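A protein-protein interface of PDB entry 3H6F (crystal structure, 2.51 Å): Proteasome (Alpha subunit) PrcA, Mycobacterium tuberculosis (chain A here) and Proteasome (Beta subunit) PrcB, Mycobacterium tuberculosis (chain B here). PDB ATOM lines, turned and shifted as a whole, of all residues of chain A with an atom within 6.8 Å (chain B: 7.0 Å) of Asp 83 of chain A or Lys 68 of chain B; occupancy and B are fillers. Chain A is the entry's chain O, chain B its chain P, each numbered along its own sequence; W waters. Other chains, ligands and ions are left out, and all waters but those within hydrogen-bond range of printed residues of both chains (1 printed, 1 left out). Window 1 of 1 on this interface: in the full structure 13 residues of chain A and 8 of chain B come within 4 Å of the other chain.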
ATOM      1  N   GLN A  51       5.775  45.560 -15.285  1.00  0.00           N
ATOM      2  CA  GLN A  51       4.451  45.093 -15.710  1.00  0.00           C
ATOM      3  C   GLN A  51       3.352  45.150 -14.638  1.00  0.00           C
ATOM      4  O   GLN A  51       3.592  44.802 -13.475  1.00  0.00           O
ATOM      5  CB  GLN A  51       4.550  43.659 -16.257  1.00  0.00           C
ATOM      6  CG  GLN A  51       4.985  42.563 -15.250  1.00  0.00           C
ATOM      7  CD  GLN A  51       5.070  41.153 -15.839  1.00  0.00           C
ATOM      8  OE1 GLN A  51       5.170  40.962 -17.057  1.00  0.00           O
ATOM      9  NE2 GLN A  51       5.059  40.156 -14.959  1.00  0.00           N
ATOM     10  N   SER A  54      -0.391  40.556 -16.168  1.00  0.00           N
ATOM     11  CA  SER A  54       0.349  39.298 -16.358  1.00  0.00           C
ATOM     12  C   SER A  54      -0.500  38.040 -16.452  1.00  0.00           C
ATOM     13  O   SER A  54      -1.661  38.019 -16.053  1.00  0.00           O
ATOM     14  CB  SER A  54       1.361  39.115 -15.216  1.00  0.00           C
ATOM     15  OG  SER A  54       2.122  37.912 -15.300  1.00  0.00           O
ATOM     16  N   GLU A  55       0.121  36.996 -16.999  1.00  0.00           N
ATOM     17  CA  GLU A  55      -0.464  35.664 -17.119  1.00  0.00           C
ATOM     18  C   GLU A  55      -0.324  34.983 -15.744  1.00  0.00           C
ATOM     19  O   GLU A  55       0.672  35.199 -15.054  1.00  0.00           O
ATOM     20  CB  GLU A  55       0.338  34.865 -18.149  1.00  0.00           C
ATOM     21  CG  GLU A  55      -0.181  33.451 -18.447  1.00  0.00           C
ATOM     22  CD  GLU A  55       0.599  32.729 -19.547  1.00  0.00           C
ATOM     23  OE1 GLU A  55       1.559  33.318 -20.104  1.00  0.00           O
ATOM     24  OE2 GLU A  55       0.248  31.560 -19.850  1.00  0.00           O
ATOM     25  N   LEU A  56      -1.354  34.267 -15.303  1.00  0.00           N
ATOM     26  CA  LEU A  56      -1.274  33.526 -14.056  1.00  0.00           C
ATOM     27  C   LEU A  56      -1.190  32.045 -14.401  1.00  0.00           C
ATOM     28  O   LEU A  56      -0.272  31.345 -13.951  1.00  0.00           O
ATOM     29  CB  LEU A  56      -2.468  33.783 -13.158  1.00  0.00           C
ATOM     30  CG  LEU A  56      -2.459  35.023 -12.280  1.00  0.00           C
ATOM     31  CD1 LEU A  56      -3.668  35.017 -11.384  1.00  0.00           C
ATOM     32  CD2 LEU A  56      -1.205  35.096 -11.444  1.00  0.00           C
ATOM     33  N   TYR A  57      -2.130  31.595 -15.234  1.00  0.00           N
ATOM     34  CA  TYR A  57      -2.205  30.217 -15.693  1.00  0.00           C
ATOM     35  C   TYR A  57      -2.839  30.187 -17.078  1.00  0.00           C
ATOM     36  O   TYR A  57      -3.051  31.226 -17.674  1.00  0.00           O
ATOM     37  CB  TYR A  57      -3.010  29.385 -14.702  1.00  0.00           C
ATOM     38  CG  TYR A  57      -2.579  27.948 -14.623  1.00  0.00           C
ATOM     39  CD1 TYR A  57      -1.339  27.597 -14.067  1.00  0.00           C
ATOM     40  CD2 TYR A  57      -3.413  26.922 -15.098  1.00  0.00           C
ATOM     41  CE1 TYR A  57      -0.932  26.251 -13.982  1.00  0.00           C
ATOM     42  CE2 TYR A  57      -3.019  25.573 -15.019  1.00  0.00           C
ATOM     43  CZ  TYR A  57      -1.780  25.252 -14.462  1.00  0.00           C
ATOM     44  OH  TYR A  57      -1.392  23.948 -14.405  1.00  0.00           O
ATOM     45  N   ASP A  58      -3.170  29.002 -17.577  1.00  0.00           N
ATOM     46  CA  ASP A  58      -3.743  28.800 -18.913  1.00  0.00           C
ATOM     47  C   ASP A  58      -4.803  29.805 -19.359  1.00  0.00           C
ATOM     48  O   ASP A  58      -4.604  30.525 -20.337  1.00  0.00           O
ATOM     49  CB  ASP A  58      -4.311  27.374 -19.048  1.00  0.00           C
ATOM     50  CG  ASP A  58      -3.239  26.282 -19.019  1.00  0.00           C
ATOM     51  OD1 ASP A  58      -2.029  26.594 -19.059  1.00  0.00           O
ATOM     52  OD2 ASP A  58      -3.620  25.088 -18.982  1.00  0.00           O
ATOM     53  N   ARG A  75       1.781  38.637  -7.499  1.00  0.00           N
ATOM     54  CA  ARG A  75       1.739  38.042  -8.832  1.00  0.00           C
ATOM     55  C   ARG A  75       2.574  36.754  -8.827  1.00  0.00           C
ATOM     56  O   ARG A  75       2.128  35.727  -9.329  1.00  0.00           O
ATOM     57  CB  ARG A  75       2.315  39.028  -9.852  1.00  0.00           C
ATOM     58  CG  ARG A  75       2.235  38.590 -11.274  1.00  0.00           C
ATOM     59  CD  ARG A  75       2.993  39.554 -12.139  1.00  0.00           C
ATOM     60  NE  ARG A  75       4.427  39.461 -11.942  1.00  0.00           N
ATOM     61  CZ  ARG A  75       5.234  38.640 -12.607  1.00  0.00           C
ATOM     62  NH1 ARG A  75       4.751  37.823 -13.536  1.00  0.00           N
ATOM     63  NH2 ARG A  75       6.528  38.629 -12.325  1.00  0.00           N
ATOM     64  N   GLY A  78       1.088  34.009  -6.747  1.00  0.00           N
ATOM     65  CA  GLY A  78      -0.076  33.467  -7.415  1.00  0.00           C
ATOM     66  C   GLY A  78       0.323  32.467  -8.476  1.00  0.00           C
ATOM     67  O   GLY A  78      -0.363  31.450  -8.654  1.00  0.00           O
ATOM     68  N   ILE A  79       1.411  32.767  -9.192  1.00  0.00           N
ATOM     69  CA  ILE A  79       1.959  31.889 -10.220  1.00  0.00           C
ATOM     70  C   ILE A  79       2.517  30.624  -9.534  1.00  0.00           C
ATOM     71  O   ILE A  79       2.327  29.514 -10.037  1.00  0.00           O
ATOM     72  CB  ILE A  79       3.042  32.621 -11.050  1.00  0.00           C
ATOM     73  CG1 ILE A  79       2.363  33.656 -11.965  1.00  0.00           C
ATOM     74  CG2 ILE A  79       3.893  31.623 -11.890  1.00  0.00           C
ATOM     75  CD1 ILE A  79       3.282  34.721 -12.542  1.00  0.00           C
ATOM     76  N   GLN A  80       3.108  30.815  -8.347  1.00  0.00           N
ATOM     77  CA  GLN A  80       3.670  29.750  -7.507  1.00  0.00           C
ATOM     78  C   GLN A  80       2.550  28.776  -7.093  1.00  0.00           C
ATOM     79  O   GLN A  80       2.681  27.565  -7.238  1.00  0.00           O
ATOM     80  CB  GLN A  80       4.305  30.386  -6.262  1.00  0.00           C
ATOM     81  CG  GLN A  80       4.984  29.453  -5.273  1.00  0.00           C
ATOM     82  CD  GLN A  80       6.311  28.942  -5.778  1.00  0.00           C
ATOM     83  OE1 GLN A  80       7.244  29.721  -5.997  1.00  0.00           O
ATOM     84  NE2 GLN A  80       6.405  27.629  -5.978  1.00  0.00           N
ATOM     85  N   PHE A  81       1.430  29.336  -6.639  1.00  0.00           N
ATOM     86  CA  PHE A  81       0.269  28.576  -6.207  1.00  0.00           C
ATOM     87  C   PHE A  81      -0.364  27.806  -7.370  1.00  0.00           C
ATOM     88  O   PHE A  81      -0.623  26.622  -7.253  1.00  0.00           O
ATOM     89  CB  PHE A  81      -0.763  29.530  -5.568  1.00  0.00           C
ATOM     90  CG  PHE A  81      -2.006  28.845  -5.063  1.00  0.00           C
ATOM     91  CD1 PHE A  81      -2.003  28.187  -3.821  1.00  0.00           C
ATOM     92  CD2 PHE A  81      -3.164  28.788  -5.864  1.00  0.00           C
ATOM     93  CE1 PHE A  81      -3.137  27.466  -3.372  1.00  0.00           C
ATOM     94  CE2 PHE A  81      -4.311  28.068  -5.437  1.00  0.00           C
ATOM     95  CZ  PHE A  81      -4.295  27.402  -4.182  1.00  0.00           C
ATOM     96  N   ALA A  82      -0.631  28.502  -8.468  1.00  0.00           N
ATOM     97  CA  ALA A  82      -1.263  27.930  -9.642  1.00  0.00           C
ATOM     98  C   ALA A  82      -0.508  26.755 -10.241  1.00  0.00           C
ATOM     99  O   ALA A  82      -1.109  25.728 -10.564  1.00  0.00           O
ATOM    100  CB  ALA A  82      -1.494  29.003 -10.691  1.00  0.00           C
ATOM    101  N   ASP A  83       0.813  26.872 -10.320  1.00  0.00           N
ATOM    102  CA  ASP A  83       1.644  25.810 -10.875  1.00  0.00           C
ATOM    103  C   ASP A  83       1.733  24.592  -9.973  1.00  0.00           C
ATOM    104  O   ASP A  83       1.716  23.467 -10.461  1.00  0.00           O
ATOM    105  CB  ASP A  83       3.025  26.343 -11.270  1.00  0.00           C
ATOM    106  CG  ASP A  83       2.989  27.146 -12.582  1.00  0.00           C
ATOM    107  OD1 ASP A  83       1.924  27.230 -13.219  1.00  0.00           O
ATOM    108  OD2 ASP A  83       4.021  27.688 -13.002  1.00  0.00           O
ATOM    109  N   THR A  84       1.669  24.825  -8.666  1.00  0.00           N
ATOM    110  CA  THR A  84       1.720  23.761  -7.669  1.00  0.00           C
ATOM    111  C   THR A  84       0.426  22.959  -7.678  1.00  0.00           C
ATOM    112  O   THR A  84       0.470  21.727  -7.650  1.00  0.00           O
ATOM    113  CB  THR A  84       2.021  24.335  -6.266  1.00  0.00           C
ATOM    114  OG1 THR A  84       3.348  24.886  -6.262  1.00  0.00           O
ATOM    115  CG2 THR A  84       1.930  23.264  -5.167  1.00  0.00           C
ATOM    116  N   ARG A  85      -0.701  23.661  -7.801  1.00  0.00           N
ATOM    117  CA  ARG A  85      -2.026  23.054  -7.849  1.00  0.00           C
ATOM    118  C   ARG A  85      -2.244  22.266  -9.109  1.00  0.00           C
ATOM    119  O   ARG A  85      -2.750  21.156  -9.043  1.00  0.00           O
ATOM    120  CB  ARG A  85      -3.116  24.119  -7.768  1.00  0.00           C
ATOM    121  CG  ARG A  85      -3.274  24.743  -6.413  1.00  0.00           C
ATOM    122  CD  ARG A  85      -3.867  23.812  -5.367  1.00  0.00           C
ATOM    123  NE  ARG A  85      -5.228  23.416  -5.703  1.00  0.00           N
ATOM    124  CZ  ARG A  85      -6.097  22.902  -4.837  1.00  0.00           C
ATOM    125  NH1 ARG A  85      -5.752  22.726  -3.572  1.00  0.00           N
ATOM    126  NH2 ARG A  85      -7.292  22.493  -5.251  1.00  0.00           N
ATOM    127  N   GLY A  86      -1.841  22.837 -10.248  1.00  0.00           N
ATOM    128  CA  GLY A  86      -2.012  22.185 -11.537  1.00  0.00           C
ATOM    129  C   GLY A  86      -1.210  20.910 -11.660  1.00  0.00           C
ATOM    130  O   GLY A  86      -1.604  19.966 -12.350  1.00  0.00           O
ATOM    131  N   TYR A  87      -0.074  20.896 -10.971  1.00  0.00           N
ATOM    132  CA  TYR A  87       0.807  19.753 -10.959  1.00  0.00           C
ATOM    133  C   TYR A  87       0.303  18.684  -9.983  1.00  0.00           C
ATOM    134  O   TYR A  87       0.347  17.502 -10.298  1.00  0.00           O
ATOM    135  CB  TYR A  87       2.231  20.182 -10.610  1.00  0.00           C
ATOM    136  CG  TYR A  87       3.234  19.072 -10.693  1.00  0.00           C
ATOM    137  CD1 TYR A  87       3.605  18.522 -11.941  1.00  0.00           C
ATOM    138  CD2 TYR A  87       3.775  18.514  -9.525  1.00  0.00           C
ATOM    139  CE1 TYR A  87       4.496  17.429 -12.026  1.00  0.00           C
ATOM    140  CE2 TYR A  87       4.672  17.418  -9.590  1.00  0.00           C
ATOM    141  CZ  TYR A  87       5.021  16.888 -10.846  1.00  0.00           C
ATOM    142  OH  TYR A  87       5.881  15.818 -10.906  1.00  0.00           O
ATOM    143  N   ALA A  88      -0.159  19.104  -8.809  1.00  0.00           N
ATOM    144  CA  ALA A  88      -0.655  18.183  -7.803  1.00  0.00           C
ATOM    145  C   ALA A  88      -2.042  17.590  -8.107  1.00  0.00           C
ATOM    146  O   ALA A  88      -2.369  16.525  -7.588  1.00  0.00           O
ATOM    147  CB  ALA A  88      -0.656  18.850  -6.446  1.00  0.00           C
ATOM    148  N   ARG A  91      -4.638  20.462 -14.637  1.00  0.00           N
ATOM    149  CA  ARG A  91      -4.591  21.839 -15.116  1.00  0.00           C
ATOM    150  C   ARG A  91      -5.940  22.532 -15.015  1.00  0.00           C
ATOM    151  O   ARG A  91      -5.984  23.735 -14.793  1.00  0.00           O
ATOM    152  CB  ARG A  91      -4.032  21.926 -16.537  1.00  0.00           C
ATOM    153  CG  ARG A  91      -2.581  21.486 -16.634  1.00  0.00           C
ATOM    154  CD  ARG A  91      -1.934  21.869 -17.961  1.00  0.00           C
ATOM    155  NE  ARG A  91      -1.526  23.281 -18.011  1.00  0.00           N
ATOM    156  CZ  ARG A  91      -0.410  23.793 -17.470  1.00  0.00           C
ATOM    157  NH1 ARG A  91       0.458  23.026 -16.816  1.00  0.00           N
ATOM    158  NH2 ARG A  91      -0.174  25.099 -17.557  1.00  0.00           N
ATOM    159  N   VAL A  94      -7.118  24.776 -11.672  1.00  0.00           N
ATOM    160  CA  VAL A  94      -6.792  26.179 -11.530  1.00  0.00           C
ATOM    161  C   VAL A  94      -7.824  27.005 -12.271  1.00  0.00           C
ATOM    162  O   VAL A  94      -7.956  26.943 -13.496  1.00  0.00           O
ATOM    163  CB  VAL A  94      -5.366  26.483 -11.997  1.00  0.00           C
ATOM    164  CG1 VAL A  94      -4.976  27.877 -11.603  1.00  0.00           C
ATOM    165  CG2 VAL A  94      -4.383  25.494 -11.396  1.00  0.00           C
ATOM    166  N   ARG A 220      -2.776  28.503 -23.813  1.00  0.00           N
ATOM    167  CA  ARG A 220      -2.403  29.764 -23.171  1.00  0.00           C
ATOM    168  C   ARG A 220      -3.144  30.942 -23.813  1.00  0.00           C
ATOM    169  O   ARG A 220      -2.803  31.393 -24.907  1.00  0.00           O
ATOM    170  CB  ARG A 220      -0.889  29.960 -23.220  1.00  0.00           C
ATOM    171  CG  ARG A 220      -0.130  28.934 -22.419  1.00  0.00           C
ATOM    172  CD  ARG A 220       1.357  29.045 -22.650  1.00  0.00           C
ATOM    173  NE  ARG A 220       1.937  30.190 -21.947  1.00  0.00           N
ATOM    174  CZ  ARG A 220       3.232  30.500 -21.946  1.00  0.00           C
ATOM    175  NH1 ARG A 220       4.109  29.751 -22.613  1.00  0.00           N
ATOM    176  NH2 ARG A 220       3.654  31.560 -21.271  1.00  0.00           N
ATOM    177  N   VAL B  61       6.456  22.297 -16.780  1.00  0.00           N
ATOM    178  CA  VAL B  61       5.929  23.187 -15.760  1.00  0.00           C
ATOM    179  C   VAL B  61       7.032  24.133 -15.326  1.00  0.00           C
ATOM    180  O   VAL B  61       6.806  25.326 -15.307  1.00  0.00           O
ATOM    181  CB  VAL B  61       5.338  22.401 -14.562  1.00  0.00           C
ATOM    182  CG1 VAL B  61       5.125  23.311 -13.312  1.00  0.00           C
ATOM    183  CG2 VAL B  61       4.002  21.790 -14.992  1.00  0.00           C
ATOM    184  N   GLU B  62       8.241  23.608 -15.113  1.00  0.00           N
ATOM    185  CA  GLU B  62       9.395  24.407 -14.701  1.00  0.00           C
ATOM    186  C   GLU B  62       9.774  25.492 -15.726  1.00  0.00           C
ATOM    187  O   GLU B  62       9.995  26.649 -15.347  1.00  0.00           O
ATOM    188  CB  GLU B  62      10.588  23.506 -14.389  1.00  0.00           C
ATOM    189  CG  GLU B  62      11.795  24.239 -13.827  1.00  0.00           C
ATOM    190  CD  GLU B  62      12.304  23.638 -12.542  1.00  0.00           C
ATOM    191  OE1 GLU B  62      11.506  23.524 -11.580  1.00  0.00           O
ATOM    192  OE2 GLU B  62      13.506  23.284 -12.499  1.00  0.00           O
ATOM    193  N   LEU B  63       9.805  25.136 -17.012  1.00  0.00           N
ATOM    194  CA  LEU B  63      10.125  26.097 -18.072  1.00  0.00           C
ATOM    195  C   LEU B  63       9.082  27.209 -18.216  1.00  0.00           C
ATOM    196  O   LEU B  63       9.451  28.368 -18.379  1.00  0.00           O
ATOM    197  CB  LEU B  63      10.305  25.403 -19.414  1.00  0.00           C
ATOM    198  CG  LEU B  63      11.466  24.412 -19.562  1.00  0.00           C
ATOM    199  CD1 LEU B  63      11.568  23.962 -21.010  1.00  0.00           C
ATOM    200  CD2 LEU B  63      12.785  25.011 -19.128  1.00  0.00           C
ATOM    201  N   GLU B  64       7.797  26.852 -18.101  1.00  0.00           N
ATOM    202  CA  GLU B  64       6.709  27.802 -18.221  1.00  0.00           C
ATOM    203  C   GLU B  64       6.569  28.653 -16.954  1.00  0.00           C
ATOM    204  O   GLU B  64       6.155  29.805 -17.027  1.00  0.00           O
ATOM    205  CB  GLU B  64       5.401  27.090 -18.549  1.00  0.00           C
ATOM    206  CG  GLU B  64       4.340  28.017 -19.130  1.00  0.00           C
ATOM    207  CD  GLU B  64       3.147  27.276 -19.675  1.00  0.00           C
ATOM    208  OE1 GLU B  64       3.240  26.778 -20.819  1.00  0.00           O
ATOM    209  OE2 GLU B  64       2.121  27.197 -18.958  1.00  0.00           O
ATOM    210  N   HIS B  65       6.979  28.099 -15.814  1.00  0.00           N
ATOM    211  CA  HIS B  65       6.930  28.789 -14.530  1.00  0.00           C
ATOM    212  C   HIS B  65       7.883  29.978 -14.583  1.00  0.00           C
ATOM    213  O   HIS B  65       7.518  31.087 -14.189  1.00  0.00           O
ATOM    214  CB  HIS B  65       7.347  27.831 -13.423  1.00  0.00           C
ATOM    215  CG  HIS B  65       7.217  28.380 -12.038  1.00  0.00           C
ATOM    216  ND1 HIS B  65       8.311  28.592 -11.226  1.00  0.00           N
ATOM    217  CD2 HIS B  65       6.129  28.655 -11.282  1.00  0.00           C
ATOM    218  CE1 HIS B  65       7.899  28.959 -10.025  1.00  0.00           C
ATOM    219  NE2 HIS B  65       6.578  29.006 -10.035  1.00  0.00           N
ATOM    220  N   TYR B  66       9.066  29.747 -15.153  1.00  0.00           N
ATOM    221  CA  TYR B  66      10.075  30.776 -15.285  1.00  0.00           C
ATOM    222  C   TYR B  66       9.604  31.864 -16.240  1.00  0.00           C
ATOM    223  O   TYR B  66       9.778  33.041 -15.949  1.00  0.00           O
ATOM    224  CB  TYR B  66      11.394  30.179 -15.767  1.00  0.00           C
ATOM    225  CG  TYR B  66      12.495  31.197 -15.924  1.00  0.00           C
ATOM    226  CD1 TYR B  66      13.381  31.482 -14.863  1.00  0.00           C
ATOM    227  CD2 TYR B  66      12.656  31.898 -17.146  1.00  0.00           C
ATOM    228  CE1 TYR B  66      14.405  32.442 -15.022  1.00  0.00           C
ATOM    229  CE2 TYR B  66      13.658  32.858 -17.312  1.00  0.00           C
ATOM    230  CZ  TYR B  66      14.530  33.126 -16.256  1.00  0.00           C
ATOM    231  OH  TYR B  66      15.501  34.079 -16.477  1.00  0.00           O
ATOM    232  N   GLU B  67       9.042  31.455 -17.376  1.00  0.00           N
ATOM    233  CA  GLU B  67       8.554  32.377 -18.395  1.00  0.00           C
ATOM    234  C   GLU B  67       7.470  33.333 -17.871  1.00  0.00           C
ATOM    235  O   GLU B  67       7.505  34.515 -18.170  1.00  0.00           O
ATOM    236  CB  GLU B  67       8.044  31.601 -19.611  1.00  0.00           C
ATOM    237  CG  GLU B  67       7.846  32.450 -20.852  1.00  0.00           C
ATOM    238  CD  GLU B  67       7.218  31.689 -22.010  1.00  0.00           C
ATOM    239  OE1 GLU B  67       7.489  30.472 -22.164  1.00  0.00           O
ATOM    240  OE2 GLU B  67       6.452  32.322 -22.777  1.00  0.00           O
ATOM    241  N   LYS B  68       6.568  32.823 -17.035  1.00  0.00           N
ATOM    242  CA  LYS B  68       5.495  33.627 -16.471  1.00  0.00           C
ATOM    243  C   LYS B  68       6.010  34.583 -15.420  1.00  0.00           C
ATOM    244  O   LYS B  68       5.555  35.718 -15.358  1.00  0.00           O
ATOM    245  CB  LYS B  68       4.400  32.748 -15.887  1.00  0.00           C
ATOM    246  CG  LYS B  68       3.577  32.039 -16.954  1.00  0.00           C
ATOM    247  CD  LYS B  68       2.385  31.257 -16.389  1.00  0.00           C
ATOM    248  CE  LYS B  68       2.776  30.056 -15.552  1.00  0.00           C
ATOM    249  NZ  LYS B  68       1.545  29.322 -15.187  1.00  0.00           N
ATOM    250  N   LEU B  69       6.986  34.126 -14.639  1.00  0.00           N
ATOM    251  CA  LEU B  69       7.594  34.916 -13.588  1.00  0.00           C
ATOM    252  C   LEU B  69       8.512  36.004 -14.100  1.00  0.00           C
ATOM    253  O   LEU B  69       8.478  37.119 -13.593  1.00  0.00           O
ATOM    254  CB  LEU B  69       8.412  34.031 -12.641  1.00  0.00           C
ATOM    255  CG  LEU B  69       7.719  33.148 -11.596  1.00  0.00           C
ATOM    256  CD1 LEU B  69       8.757  32.388 -10.821  1.00  0.00           C
ATOM    257  CD2 LEU B  69       6.873  33.959 -10.633  1.00  0.00           C
ATOM    258  N   GLU B  70       9.331  35.681 -15.095  1.00  0.00           N
ATOM    259  CA  GLU B  70      10.310  36.632 -15.614  1.00  0.00           C
ATOM    260  C   GLU B  70       9.977  37.310 -16.922  1.00  0.00           C
ATOM    261  O   GLU B  70      10.710  38.202 -17.340  1.00  0.00           O
ATOM    262  CB  GLU B  70      11.711  35.992 -15.682  1.00  0.00           C
ATOM    263  CG  GLU B  70      12.176  35.262 -14.397  1.00  0.00           C
ATOM    264  CD  GLU B  70      12.175  36.108 -13.101  1.00  0.00           C
ATOM    265  OE1 GLU B  70      12.608  37.291 -13.114  1.00  0.00           O
ATOM    266  OE2 GLU B  70      11.754  35.567 -12.050  1.00  0.00           O
ATOM    267  N   GLY B  71       8.906  36.877 -17.577  1.00  0.00           N
ATOM    268  CA  GLY B  71       8.488  37.501 -18.818  1.00  0.00           C
ATOM    269  C   GLY B  71       9.114  36.997 -20.096  1.00  0.00           C
ATOM    270  O   GLY B  71       8.558  37.235 -21.172  1.00  0.00           O
ATOM    271  N   VAL B  72      10.283  36.364 -19.994  1.00  0.00           N
ATOM    272  CA  VAL B  72      11.005  35.816 -21.156  1.00  0.00           C
ATOM    273  C   VAL B  72      11.390  34.352 -20.890  1.00  0.00           C
ATOM    274  O   VAL B  72      11.503  33.947 -19.727  1.00  0.00           O
ATOM    275  CB  VAL B  72      12.336  36.622 -21.446  1.00  0.00           C
ATOM    276  CG1 VAL B  72      12.017  38.013 -22.002  1.00  0.00           C
ATOM    277  CG2 VAL B  72      13.220  36.712 -20.195  1.00  0.00           C
HETATM  278  O   HOH W   1       0.098  29.435 -18.327  1.00  0.00           O
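NH2 of Arg 220 of chain A lies within salt-bridge range of OE2 of Glu 67 of chain B. OE1 of Glu 64 of chain B lies within salt-bridge range of NH1 of Arg 220 of chain A (3.6 Å). The backbone carbonyl oxygen of Leu 56 of chain A is in hydrogen-bond range of the side-chain amino group of Lys 68 of chain B, at 3.0 Å. OD1 of Asp 83 of chain A lies within salt-bridge range of NZ of Lys 68 of chain B (2.9 Å). NH1 of Arg 75 of chain A is in hydrogen-bond range of O of Lys 68 of chain B (2.9 Å). The guanidinium group (NH2) of Arg 91 of chain A is in salt-bridge range of the side-chain carboxylate (OE2) of Glu 64 of chain B, at 3.4 Å. NH2 of Arg 75 of chain A lies within hydrogen-bond range of O of Leu 69 of chain B, at 2.8 Å.
The side-chain carboxylate of Asp 58 of chain A is in salt-bridge range of the guanidinium group of Arg 91 of chain A. O of Gln 80 of chain A sits at hydrogen-bond distance from OG1 of Thr 84 of chain A (2.9 Å). The guanidinium group (NH1) of Arg 91 of chain A is in hydrogen-bond range of the side-chain hydroxyl (OH) of Tyr 57 of chain A (3.2 Å). The side-chain carboxylate (OE1) of Glu 55 of chain A lies within salt-bridge range of the guanidinium group (NH2) of Arg 220 of chain A (3.0 Å). The guanidinium group (NH1) of Arg 75 of chain A is in hydrogen-bond range of the side-chain hydroxyl (OG) of Ser 54 of chain A, at 3.2 Å. The guanidinium group of Arg 75 of chain A lies close to the side-chain amide nitrogen of Gln 51 of chain A.
Among the printed residues, pairs that only touch across the chains: Glu 55 of chain A with Lys 68 of chain B (3.9 Å), Tyr 57 of chain A with Lys 68 of chain B (3.5 Å), Ile 79 of chain A with His 65 of chain B (3.8 Å), Ile 79 of chain A with Lys 68 of chain B (3.8 Å), Ile 79 of chain A with Leu 69 of chain B (3.99 Å), Gln 80 of chain A with His 65 of chain B (3.9 Å) and Asp 83 of chain A with His 65 of chain B (2.9 Å).
Printed residues of chain B within 4 Å of Glu 55 of chain A: Lys 68 (3.9 Å). Of the printed residues of chain B, Ile 79 of chain A touches His 65 (3.8 Å), Lys 68 (3.8 Å) and Leu 69 (3.99 Å). Asp 83 of chain A touches just these residues of chain B: His 65 (2.9 Å) and Lys 68 (2.9 Å). Of the printed residues of chain B, Arg 91 of chain A touches Glu 64. Glu 62 of chain B touches none of the printed residues of chain A. Lys 68 of chain B touches just these residues of chain A: Glu 55, Leu 56, Tyr 57, Arg 75, Ile 79 and Asp 83. Of the printed residues of chain A, Leu 69 of chain B touches Arg 75 and Ile 79. The nearest residue of chain B that does not touch Asp 83 of chain A is Val 61 of chain B (4.2 Å). The nearest residue of chain A that does not touch Lys 68 of chain B is Ser 54 of chain A (4.1 Å).
Of the 21 printed residues of chain A, 9 touch a printed residue of chain B. Of the 12 printed residues of chain B, 5 touch a printed residue of chain A. Hydrophobic or aromatic side chains of chain B within 4 Å of the printed part of chain A: His 65 and Leu 69. Among the printed residues, 14 pairs touch across the chains.
Water W1 lies within hydrogen-bond range of the side-chain carboxylate (OE2) of Glu 55 of chain A (2.6 Å), the side-chain carboxylate (OE2) of Glu 64 of chain B (3.1 Å), the backbone NH (N) of Asp 58 of chain A (3.4 Å) and the side-chain amino group (NZ) of Lys 68 of chain B (3.5 Å).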
